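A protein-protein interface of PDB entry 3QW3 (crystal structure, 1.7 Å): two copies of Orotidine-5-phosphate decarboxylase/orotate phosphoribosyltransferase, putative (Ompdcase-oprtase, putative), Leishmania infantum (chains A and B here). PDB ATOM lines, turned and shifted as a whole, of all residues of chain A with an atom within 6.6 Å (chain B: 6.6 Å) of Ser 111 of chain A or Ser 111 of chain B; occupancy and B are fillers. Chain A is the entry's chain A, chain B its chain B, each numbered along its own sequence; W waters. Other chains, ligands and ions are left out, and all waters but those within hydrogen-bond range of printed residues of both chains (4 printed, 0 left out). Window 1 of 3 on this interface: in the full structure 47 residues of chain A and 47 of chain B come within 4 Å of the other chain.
Water W4 bridges O of Lys 84 of chain A (2.7 Å) and O of Lys 84 of chain B (2.8 Å). Water W1 bridges O of Gly 86 of chain B (2.8 Å) and O of Lys 84 of chain A (3.5 Å). Water W2 lies within hydrogen-bond range of O of Lys 84 of chain B and N of Gly 86 of chain A. Water W3 bridges the backbone NH (N) of Gly 86 of chain B and the backbone carbonyl oxygen (O) of Lys 84 of chain A.
Printed residues of chain A that touch a printed residue of chain B: Lys 84, Arg 85, Gly 86, Asp 87, Ser 111, Pro 112, Tyr 113, Met 114 and Leu 133. Hydrophobic or aromatic side chains of chain A that line the printed part of chain B: Pro 112, Tyr 113, Met 114 and Leu 133. Of the 16 printed residues of chain B, 9 touch a printed residue of chain A. Hydrophobic or aromatic side chains of chain B that line the printed part of chain A: Pro 112, Tyr 113, Met 114 and Leu 133. Among the printed residues, 12 pairs touch across the chains. Among the printed residues, Asp or Glu carboxylates within 4 Å of a Lys or Arg side-chain nitrogen of the other chain: Lys 84 of chain A with Asp 87 of chain B and Asp 87 of chain A with Lys 84 of chain B.
Of the printed residues of chain B, Ser 111 of chain A touches Ser 111. Of chain A, only Ser 111 comes within 4 Å of Ser 111 of chain B. Printed residues of chain B within 4 Å of Leu 133 of chain A: Tyr 113 (3.6 Å) and Met 114 (3.95 Å). Of the printed residues of chain A, Tyr 113 of chain B touches Pro 112 (3.9 Å) and Leu 133 (3.6 Å). Of the printed residues of chain A, Leu 133 of chain B touches Tyr 113. Of the printed residues of chain B, Arg 85 of chain A touches Arg 85 (3.6 Å). Printed residues of chain B within 4 Å of Pro 112 of chain A: Tyr 113. Phe 131 of chain A touches none of the printed residues of chain B. The nearest printed residue of chain B that does not touch Gly 86 of chain A is Leu 133 of chain B (5.1 Å).
Among the printed residues, pairs that only touch across the chains: Lys 84 of chain A with Gly 86 of chain B, Arg 85 of chain A with Arg 85 of chain B, Gly 86 of chain A with Lys 84 of chain B, Pro 112 of chain A with Tyr 113 of chain B, Tyr 113 of chain A with Pro 112 of chain B, Tyr 113 of chain A with Leu 133 of chain B, Met 114 of chain A with Lys 84 of chain B, Leu 133 of chain A with Tyr 113 of chain B and Leu 133 of chain A with Met 114 of chain B.
The backbone NH (N) of Arg 85 of chain A sits at hydrogen-bond distance from the backbone carbonyl oxygen (O) of Thr 109 of chain A, 3.1 Å away. The backbone NH (N) of Ser 111 of chain A lies within hydrogen-bond range of the backbone carbonyl oxygen (O) of Arg 85 of chain A (3.0 Å). The side-chain hydroxyl (OG1) of Thr 109 of chain B lies within hydrogen-bond range of the backbone NH (N) of Lys 84 of chain B, at 2.9 Å. The backbone NH (N) of Arg 85 of chain B is in hydrogen-bond range of the backbone carbonyl oxygen (O) of Thr 109 of chain B, at 3.1 Å. The backbone carbonyl oxygen (O) of Arg 85 of chain B is in hydrogen-bond range of the backbone NH (N) of Ser 111 of chain B (3.0 Å). N of Tyr 113 of chain B is in hydrogen-bond range of OG of Ser 111 of chain B, at 3.2 Å.
The side-chain carboxylate (OD1) of Asp 87 of chain B lies within salt-bridge range of the side-chain amino group (NZ) of Lys 84 of chain A, at 2.9 Å. The side-chain carboxylate (OD1) of Asp 87 of chain A lies within salt-bridge range of the side-chain amino group (NZ) of Lys 84 of chain B (2.8 Å). The side-chain hydroxyl (OG) of Ser 111 of chain A sits at hydrogen-bond distance from the side-chain hydroxyl (OG) of Ser 111 of chain B.
Lys 84 of chain A touches Gly 86 of chain B, and with the chains exchanged Gly 86 of chain A touches Lys 84 of chain B. Arg 85 of chain B touches its own counterpart, Arg 85 of chain A. Ser 111 of chain A touches its own counterpart, Ser 111 of chain B. Tyr 113 of chain A touches Leu 133 of chain B, and with the chains exchanged Leu 133 of chain A touches Tyr 113 of chain B. Of the 12 pairs that touch across the chains among the printed residues, 10 have their exchanged pair printed and touching as well.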
ATOM      1  N   LYS A  84       4.606  19.442  17.646  1.00  0.00           N
ATOM      2  CA  LYS A  84       3.519  20.091  18.391  1.00  0.00           C
ATOM      3  C   LYS A  84       3.794  21.587  18.623  1.00  0.00           C
ATOM      4  O   LYS A  84       3.824  22.074  19.753  1.00  0.00           O
ATOM      5  CB  LYS A  84       3.209  19.328  19.692  1.00  0.00           C
ATOM      6  CG  LYS A  84       2.759  17.877  19.448  1.00  0.00           C
ATOM      7  CD  LYS A  84       2.373  17.160  20.746  1.00  0.00           C
ATOM      8  CE  LYS A  84       1.906  15.715  20.495  1.00  0.00           C
ATOM      9  NZ  LYS A  84       3.014  14.805  20.060  1.00  0.00           N
ATOM     10  N   ARG A  85       3.995  22.305  17.522  1.00  0.00           N
ATOM     11  CA  ARG A  85       4.311  23.725  17.580  1.00  0.00           C
ATOM     12  C   ARG A  85       3.053  24.579  17.662  1.00  0.00           C
ATOM     13  O   ARG A  85       1.961  24.154  17.281  1.00  0.00           O
ATOM     14  CB  ARG A  85       5.154  24.139  16.366  1.00  0.00           C
ATOM     15  CG  ARG A  85       6.486  23.391  16.211  1.00  0.00           C
ATOM     16  CD  ARG A  85       7.448  23.626  17.388  1.00  0.00           C
ATOM     17  NE  ARG A  85       8.838  23.290  17.067  1.00  0.00           N
ATOM     18  CZ  ARG A  85       9.577  22.375  17.698  1.00  0.00           C
ATOM     19  NH1 ARG A  85       9.070  21.650  18.690  1.00  0.00           N
ATOM     20  NH2 ARG A  85      10.839  22.180  17.329  1.00  0.00           N
ATOM     21  N   GLY A  86       3.205  25.797  18.164  1.00  0.00           N
ATOM     22  CA  GLY A  86       2.100  26.741  18.168  1.00  0.00           C
ATOM     23  C   GLY A  86       2.597  28.084  18.641  1.00  0.00           C
ATOM     24  O   GLY A  86       3.029  28.221  19.779  1.00  0.00           O
ATOM     25  N   ASP A  87       2.550  29.067  17.751  1.00  0.00           N
ATOM     26  CA  ASP A  87       2.944  30.432  18.087  1.00  0.00           C
ATOM     27  C   ASP A  87       2.297  31.335  17.057  1.00  0.00           C
ATOM     28  O   ASP A  87       1.462  30.884  16.292  1.00  0.00           O
ATOM     29  CB  ASP A  87       4.470  30.579  18.072  1.00  0.00           C
ATOM     30  CG  ASP A  87       4.973  31.609  19.078  1.00  0.00           C
ATOM     31  OD1 ASP A  87       5.855  31.268  19.894  1.00  0.00           O
ATOM     32  OD2 ASP A  87       4.492  32.757  19.061  1.00  0.00           O
ATOM     33  N   THR A 109       2.935  18.416  13.462  1.00  0.00           N
ATOM     34  CA  THR A 109       1.853  18.461  14.444  1.00  0.00           C
ATOM     35  C   THR A 109       1.829  19.835  15.113  1.00  0.00           C
ATOM     36  O   THR A 109       2.861  20.487  15.229  1.00  0.00           O
ATOM     37  CB  THR A 109       1.992  17.365  15.513  1.00  0.00           C
ATOM     38  OG1 THR A 109       3.310  17.409  16.073  1.00  0.00           O
ATOM     39  CG2 THR A 109       1.746  15.987  14.893  1.00  0.00           C
ATOM     40  N   ALA A 110       0.648  20.266  15.538  1.00  0.00           N
ATOM     41  CA  ALA A 110       0.479  21.623  16.070  1.00  0.00           C
ATOM     42  C   ALA A 110      -0.609  21.689  17.128  1.00  0.00           C
ATOM     43  O   ALA A 110      -1.587  20.941  17.063  1.00  0.00           O
ATOM     44  CB  ALA A 110       0.167  22.598  14.940  1.00  0.00           C
ATOM     45  N   SER A 111      -0.427  22.591  18.093  1.00  0.00           N
ATOM     46  CA  SER A 111      -1.423  22.851  19.133  1.00  0.00           C
ATOM     47  C   SER A 111      -2.479  23.830  18.608  1.00  0.00           C
ATOM     48  O   SER A 111      -2.139  24.774  17.896  1.00  0.00           O
ATOM     49  CB  SER A 111      -0.740  23.437  20.382  1.00  0.00           C
ATOM     50  OG  SER A 111      -1.697  24.020  21.259  1.00  0.00           O
ATOM     51  N   PRO A 112      -3.756  23.621  18.974  1.00  0.00           N
ATOM     52  CA  PRO A 112      -4.828  24.521  18.560  1.00  0.00           C
ATOM     53  C   PRO A 112      -5.037  25.715  19.484  1.00  0.00           C
ATOM     54  O   PRO A 112      -5.853  26.581  19.164  1.00  0.00           O
ATOM     55  CB  PRO A 112      -6.066  23.626  18.642  1.00  0.00           C
ATOM     56  CG  PRO A 112      -5.762  22.717  19.782  1.00  0.00           C
ATOM     57  CD  PRO A 112      -4.285  22.430  19.664  1.00  0.00           C
ATOM     58  N   TYR A 113      -4.318  25.767  20.609  1.00  0.00           N
ATOM     59  CA  TYR A 113      -4.683  26.703  21.689  1.00  0.00           C
ATOM     60  C   TYR A 113      -4.718  28.189  21.302  1.00  0.00           C
ATOM     61  O   TYR A 113      -5.571  28.935  21.799  1.00  0.00           O
ATOM     62  CB  TYR A 113      -3.861  26.491  22.972  1.00  0.00           C
ATOM     63  CG  TYR A 113      -4.465  27.240  24.152  1.00  0.00           C
ATOM     64  CD1 TYR A 113      -3.912  28.440  24.602  1.00  0.00           C
ATOM     65  CD2 TYR A 113      -5.618  26.767  24.781  1.00  0.00           C
ATOM     66  CE1 TYR A 113      -4.485  29.138  25.671  1.00  0.00           C
ATOM     67  CE2 TYR A 113      -6.193  27.454  25.848  1.00  0.00           C
ATOM     68  CZ  TYR A 113      -5.622  28.634  26.283  1.00  0.00           C
ATOM     69  OH  TYR A 113      -6.213  29.310  27.328  1.00  0.00           O
ATOM     70  N   MET A 114      -3.814  28.613  20.427  1.00  0.00           N
ATOM     71  CA  MET A 114      -3.769  30.022  20.022  1.00  0.00           C
ATOM     72  C   MET A 114      -4.647  30.324  18.799  1.00  0.00           C
ATOM     73  O   MET A 114      -4.668  31.455  18.306  1.00  0.00           O
ATOM     74  CB  MET A 114      -2.327  30.476  19.817  1.00  0.00           C
ATOM     75  CG  MET A 114      -1.526  30.499  21.113  1.00  0.00           C
ATOM     76  SD  MET A 114       0.208  30.892  20.878  1.00  0.00           S
ATOM     77  CE  MET A 114       0.118  32.637  20.475  1.00  0.00           C
ATOM     78  N   GLY A 115      -5.363  29.313  18.317  1.00  0.00           N
ATOM     79  CA  GLY A 115      -6.404  29.517  17.303  1.00  0.00           C
ATOM     80  C   GLY A 115      -5.939  29.702  15.873  1.00  0.00           C
ATOM     81  O   GLY A 115      -4.783  29.448  15.547  1.00  0.00           O
ATOM     82  N   SER A 118      -2.602  31.298  14.537  1.00  0.00           N
ATOM     83  CA  SER A 118      -1.431  30.556  14.990  1.00  0.00           C
ATOM     84  C   SER A 118      -1.216  29.295  14.153  1.00  0.00           C
ATOM     85  O   SER A 118      -0.135  28.699  14.179  1.00  0.00           O
ATOM     86  CB  SER A 118      -1.549  30.201  16.473  1.00  0.00           C
ATOM     87  OG  SER A 118      -2.484  29.160  16.688  1.00  0.00           O
ATOM     88  N   LEU A 119      -2.251  28.898  13.413  1.00  0.00           N
ATOM     89  CA  LEU A 119      -2.188  27.710  12.557  1.00  0.00           C
ATOM     90  C   LEU A 119      -1.972  28.051  11.083  1.00  0.00           C
ATOM     91  O   LEU A 119      -1.330  27.293  10.358  1.00  0.00           O
ATOM     92  CB  LEU A 119      -3.457  26.868  12.738  1.00  0.00           C
ATOM     93  CG  LEU A 119      -3.651  26.244  14.125  1.00  0.00           C
ATOM     94  CD1 LEU A 119      -5.048  25.641  14.253  1.00  0.00           C
ATOM     95  CD2 LEU A 119      -2.572  25.201  14.415  1.00  0.00           C
ATOM     96  N   PHE A 131      -1.293  18.454  11.303  1.00  0.00           N
ATOM     97  CA  PHE A 131      -2.107  17.645  12.196  1.00  0.00           C
ATOM     98  C   PHE A 131      -2.277  18.382  13.518  1.00  0.00           C
ATOM     99  O   PHE A 131      -1.318  18.551  14.270  1.00  0.00           O
ATOM    100  CB  PHE A 131      -1.462  16.275  12.408  1.00  0.00           C
ATOM    101  CG  PHE A 131      -1.584  15.362  11.214  1.00  0.00           C
ATOM    102  CD1 PHE A 131      -2.736  14.606  11.032  1.00  0.00           C
ATOM    103  CD2 PHE A 131      -0.549  15.258  10.290  1.00  0.00           C
ATOM    104  CE1 PHE A 131      -2.868  13.751   9.928  1.00  0.00           C
ATOM    105  CE2 PHE A 131      -0.670  14.405   9.172  1.00  0.00           C
ATOM    106  CZ  PHE A 131      -1.835  13.658   9.000  1.00  0.00           C
ATOM    107  N   VAL A 132      -3.503  18.824  13.784  1.00  0.00           N
ATOM    108  CA  VAL A 132      -3.798  19.654  14.955  1.00  0.00           C
ATOM    109  C   VAL A 132      -4.251  18.789  16.117  1.00  0.00           C
ATOM    110  O   VAL A 132      -5.116  17.927  15.955  1.00  0.00           O
ATOM    111  CB  VAL A 132      -4.887  20.705  14.636  1.00  0.00           C
ATOM    112  CG1 VAL A 132      -5.125  21.605  15.849  1.00  0.00           C
ATOM    113  CG2 VAL A 132      -4.469  21.543  13.438  1.00  0.00           C
ATOM    114  N   LEU A 133      -3.673  19.020  17.293  1.00  0.00           N
ATOM    115  CA  LEU A 133      -4.070  18.264  18.482  1.00  0.00           C
ATOM    116  C   LEU A 133      -5.561  18.398  18.718  1.00  0.00           C
ATOM    117  O   LEU A 133      -6.106  19.504  18.678  1.00  0.00           O
ATOM    118  CB  LEU A 133      -3.306  18.748  19.716  1.00  0.00           C
ATOM    119  CG  LEU A 133      -1.782  18.784  19.648  1.00  0.00           C
ATOM    120  CD1 LEU A 133      -1.246  19.304  20.994  1.00  0.00           C
ATOM    121  CD2 LEU A 133      -1.203  17.414  19.337  1.00  0.00           C
ATOM    122  N   LYS B  84       7.080  27.481  23.755  1.00  0.00           N
ATOM    123  CA  LYS B  84       5.665  27.050  23.737  1.00  0.00           C
ATOM    124  C   LYS B  84       5.528  25.540  23.470  1.00  0.00           C
ATOM    125  O   LYS B  84       4.913  25.106  22.484  1.00  0.00           O
ATOM    126  CB  LYS B  84       4.833  27.886  22.745  1.00  0.00           C
ATOM    127  CG  LYS B  84       4.750  29.387  23.103  1.00  0.00           C
ATOM    128  CD  LYS B  84       3.795  30.160  22.186  1.00  0.00           C
ATOM    129  CE  LYS B  84       3.719  31.656  22.541  1.00  0.00           C
ATOM    130  NZ  LYS B  84       5.018  32.386  22.353  1.00  0.00           N
ATOM    131  N   ARG B  85       6.124  24.747  24.351  1.00  0.00           N
ATOM    132  CA  ARG B  85       6.181  23.301  24.161  1.00  0.00           C
ATOM    133  C   ARG B  85       4.973  22.637  24.793  1.00  0.00           C
ATOM    134  O   ARG B  85       4.351  23.174  25.704  1.00  0.00           O
ATOM    135  CB  ARG B  85       7.469  22.721  24.763  1.00  0.00           C
ATOM    136  CG  ARG B  85       8.776  23.246  24.143  1.00  0.00           C
ATOM    137  CD  ARG B  85       8.872  22.940  22.652  1.00  0.00           C
ATOM    138  NE  ARG B  85      10.237  23.052  22.141  1.00  0.00           N
ATOM    139  CZ  ARG B  85      10.632  23.852  21.152  1.00  0.00           C
ATOM    140  NH1 ARG B  85       9.782  24.676  20.545  1.00  0.00           N
ATOM    141  NH2 ARG B  85      11.904  23.829  20.772  1.00  0.00           N
ATOM    142  N   GLY B  86       4.637  21.450  24.313  1.00  0.00           N
ATOM    143  CA  GLY B  86       3.586  20.675  24.957  1.00  0.00           C
ATOM    144  C   GLY B  86       3.544  19.287  24.375  1.00  0.00           C
ATOM    145  O   GLY B  86       3.234  19.116  23.205  1.00  0.00           O
ATOM    146  N   ASP B  87       3.874  18.300  25.199  1.00  0.00           N
ATOM    147  CA  ASP B  87       3.836  16.906  24.779  1.00  0.00           C
ATOM    148  C   ASP B  87       3.739  16.082  26.047  1.00  0.00           C
ATOM    149  O   ASP B  87       3.472  16.627  27.114  1.00  0.00           O
ATOM    150  CB  ASP B  87       5.088  16.544  23.970  1.00  0.00           C
ATOM    151  CG  ASP B  87       4.813  15.490  22.904  1.00  0.00           C
ATOM    152  OD1 ASP B  87       5.185  15.708  21.729  1.00  0.00           O
ATOM    153  OD2 ASP B  87       4.224  14.441  23.235  1.00  0.00           O
ATOM    154  N   THR B 109       7.939  28.587  28.149  1.00  0.00           N
ATOM    155  CA  THR B 109       6.508  28.720  27.914  1.00  0.00           C
ATOM    156  C   THR B 109       5.962  27.386  27.420  1.00  0.00           C
ATOM    157  O   THR B 109       6.689  26.608  26.800  1.00  0.00           O
ATOM    158  CB  THR B 109       6.203  29.807  26.901  1.00  0.00           C
ATOM    159  OG1 THR B 109       7.037  29.612  25.752  1.00  0.00           O
ATOM    160  CG2 THR B 109       6.486  31.179  27.508  1.00  0.00           C
ATOM    161  N   ALA B 110       4.700  27.118  27.728  1.00  0.00           N
ATOM    162  CA  ALA B 110       4.097  25.821  27.437  1.00  0.00           C
ATOM    163  C   ALA B 110       2.610  25.942  27.139  1.00  0.00           C
ATOM    164  O   ALA B 110       1.921  26.790  27.710  1.00  0.00           O
ATOM    165  CB  ALA B 110       4.329  24.857  28.596  1.00  0.00           C
ATOM    166  N   SER B 111       2.130  25.085  26.239  1.00  0.00           N
ATOM    167  CA  SER B 111       0.709  25.002  25.915  1.00  0.00           C
ATOM    168  C   SER B 111      -0.032  24.178  26.972  1.00  0.00           C
ATOM    169  O   SER B 111       0.477  23.160  27.435  1.00  0.00           O
ATOM    170  CB  SER B 111       0.518  24.370  24.528  1.00  0.00           C
ATOM    171  OG  SER B 111      -0.840  24.007  24.334  1.00  0.00           O
ATOM    172  N   PRO B 112      -1.243  24.618  27.357  1.00  0.00           N
ATOM    173  CA  PRO B 112      -2.051  23.889  28.321  1.00  0.00           C
ATOM    174  C   PRO B 112      -2.908  22.785  27.696  1.00  0.00           C
ATOM    175  O   PRO B 112      -3.575  22.051  28.430  1.00  0.00           O
ATOM    176  CB  PRO B 112      -2.979  24.978  28.865  1.00  0.00           C
ATOM    177  CG  PRO B 112      -3.213  25.865  27.679  1.00  0.00           C
ATOM    178  CD  PRO B 112      -1.908  25.862  26.908  1.00  0.00           C
ATOM    179  N   TYR B 113      -2.893  22.661  26.367  1.00  0.00           N
ATOM    180  CA  TYR B 113      -3.925  21.860  25.690  1.00  0.00           C
ATOM    181  C   TYR B 113      -3.981  20.374  26.082  1.00  0.00           C
ATOM    182  O   TYR B 113      -5.070  19.782  26.123  1.00  0.00           O
ATOM    183  CB  TYR B 113      -3.880  22.029  24.162  1.00  0.00           C
ATOM    184  CG  TYR B 113      -5.106  21.436  23.514  1.00  0.00           C
ATOM    185  CD1 TYR B 113      -5.052  20.197  22.859  1.00  0.00           C
ATOM    186  CD2 TYR B 113      -6.338  22.083  23.608  1.00  0.00           C
ATOM    187  CE1 TYR B 113      -6.200  19.636  22.292  1.00  0.00           C
ATOM    188  CE2 TYR B 113      -7.489  21.538  23.038  1.00  0.00           C
ATOM    189  CZ  TYR B 113      -7.412  20.317  22.384  1.00  0.00           C
ATOM    190  OH  TYR B 113      -8.560  19.794  21.842  1.00  0.00           O
ATOM    191  N   MET B 114      -2.825  19.784  26.380  1.00  0.00           N
ATOM    192  CA  MET B 114      -2.774  18.375  26.757  1.00  0.00           C
ATOM    193  C   MET B 114      -2.900  18.144  28.264  1.00  0.00           C
ATOM    194  O   MET B 114      -2.861  17.003  28.725  1.00  0.00           O
ATOM    195  CB  MET B 114      -1.533  17.698  26.167  1.00  0.00           C
ATOM    196  CG  MET B 114      -1.625  17.564  24.663  1.00  0.00           C
ATOM    197  SD  MET B 114      -0.146  16.880  23.916  1.00  0.00           S
ATOM    198  CE  MET B 114      -0.208  15.182  24.513  1.00  0.00           C
ATOM    199  N   GLY B 115      -3.054  19.227  29.022  1.00  0.00           N
ATOM    200  CA  GLY B 115      -3.373  19.135  30.452  1.00  0.00           C
ATOM    201  C   GLY B 115      -2.226  18.843  31.407  1.00  0.00           C
ATOM    202  O   GLY B 115      -1.050  18.957  31.049  1.00  0.00           O
ATOM    203  N   SER B 118       0.969  16.651  30.776  1.00  0.00           N
ATOM    204  CA  SER B 118       1.815  17.239  29.745  1.00  0.00           C
ATOM    205  C   SER B 118       2.667  18.364  30.326  1.00  0.00           C
ATOM    206  O   SER B 118       3.740  18.668  29.808  1.00  0.00           O
ATOM    207  CB  SER B 118       1.005  17.731  28.536  1.00  0.00           C
ATOM    208  OG  SER B 118       0.218  18.869  28.836  1.00  0.00           O
ATOM    209  N   LEU B 119       2.190  18.965  31.416  1.00  0.00           N
ATOM    210  CA  LEU B 119       2.870  20.105  32.019  1.00  0.00           C
ATOM    211  C   LEU B 119       3.823  19.681  33.131  1.00  0.00           C
ATOM    212  O   LEU B 119       4.851  20.321  33.349  1.00  0.00           O
ATOM    213  CB  LEU B 119       1.841  21.117  32.544  1.00  0.00           C
ATOM    214  CG  LEU B 119       1.028  21.821  31.453  1.00  0.00           C
ATOM    215  CD1 LEU B 119      -0.167  22.538  32.056  1.00  0.00           C
ATOM    216  CD2 LEU B 119       1.886  22.803  30.653  1.00  0.00           C
ATOM    217  N   PHE B 131       5.650  29.123  32.214  1.00  0.00           N
ATOM    218  CA  PHE B 131       4.596  30.067  31.865  1.00  0.00           C
ATOM    219  C   PHE B 131       3.617  29.415  30.895  1.00  0.00           C
ATOM    220  O   PHE B 131       3.956  29.161  29.738  1.00  0.00           O
ATOM    221  CB  PHE B 131       5.208  31.330  31.256  1.00  0.00           C
ATOM    222  CG  PHE B 131       5.882  32.210  32.272  1.00  0.00           C
ATOM    223  CD1 PHE B 131       5.127  33.122  33.015  1.00  0.00           C
ATOM    224  CD2 PHE B 131       7.254  32.110  32.506  1.00  0.00           C
ATOM    225  CE1 PHE B 131       5.731  33.928  33.974  1.00  0.00           C
ATOM    226  CE2 PHE B 131       7.877  32.920  33.469  1.00  0.00           C
ATOM    227  CZ  PHE B 131       7.105  33.831  34.200  1.00  0.00           C
ATOM    228  N   VAL B 132       2.411  29.135  31.380  1.00  0.00           N
ATOM    229  CA  VAL B 132       1.419  28.415  30.586  1.00  0.00           C
ATOM    230  C   VAL B 132       0.559  29.391  29.796  1.00  0.00           C
ATOM    231  O   VAL B 132       0.056  30.369  30.357  1.00  0.00           O
ATOM    232  CB  VAL B 132       0.533  27.522  31.476  1.00  0.00           C
ATOM    233  CG1 VAL B 132      -0.479  26.740  30.624  1.00  0.00           C
ATOM    234  CG2 VAL B 132       1.397  26.562  32.284  1.00  0.00           C
ATOM    235  N   LEU B 133       0.399  29.128  28.498  1.00  0.00           N
ATOM    236  CA  LEU B 133      -0.464  29.961  27.654  1.00  0.00           C
ATOM    237  C   LEU B 133      -1.855  30.063  28.244  1.00  0.00           C
ATOM    238  O   LEU B 133      -2.461  29.050  28.605  1.00  0.00           O
ATOM    239  CB  LEU B 133      -0.555  29.396  26.232  1.00  0.00           C
ATOM    240  CG  LEU B 133       0.763  29.130  25.512  1.00  0.00           C
ATOM    241  CD1 LEU B 133       0.455  28.561  24.132  1.00  0.00           C
ATOM    242  CD2 LEU B 133       1.610  30.399  25.403  1.00  0.00           C
HETATM  243  O   HOH W   1       1.603  21.207  22.315  1.00  0.00           O
HETATM  244  O   HOH W   2       5.671  25.850  19.821  1.00  0.00           O
HETATM  245  O   HOH W   3       5.862  21.068  21.696  1.00  0.00           O
HETATM  246  O   HOH W   4       2.661  23.719  21.547  1.00  0.00           O
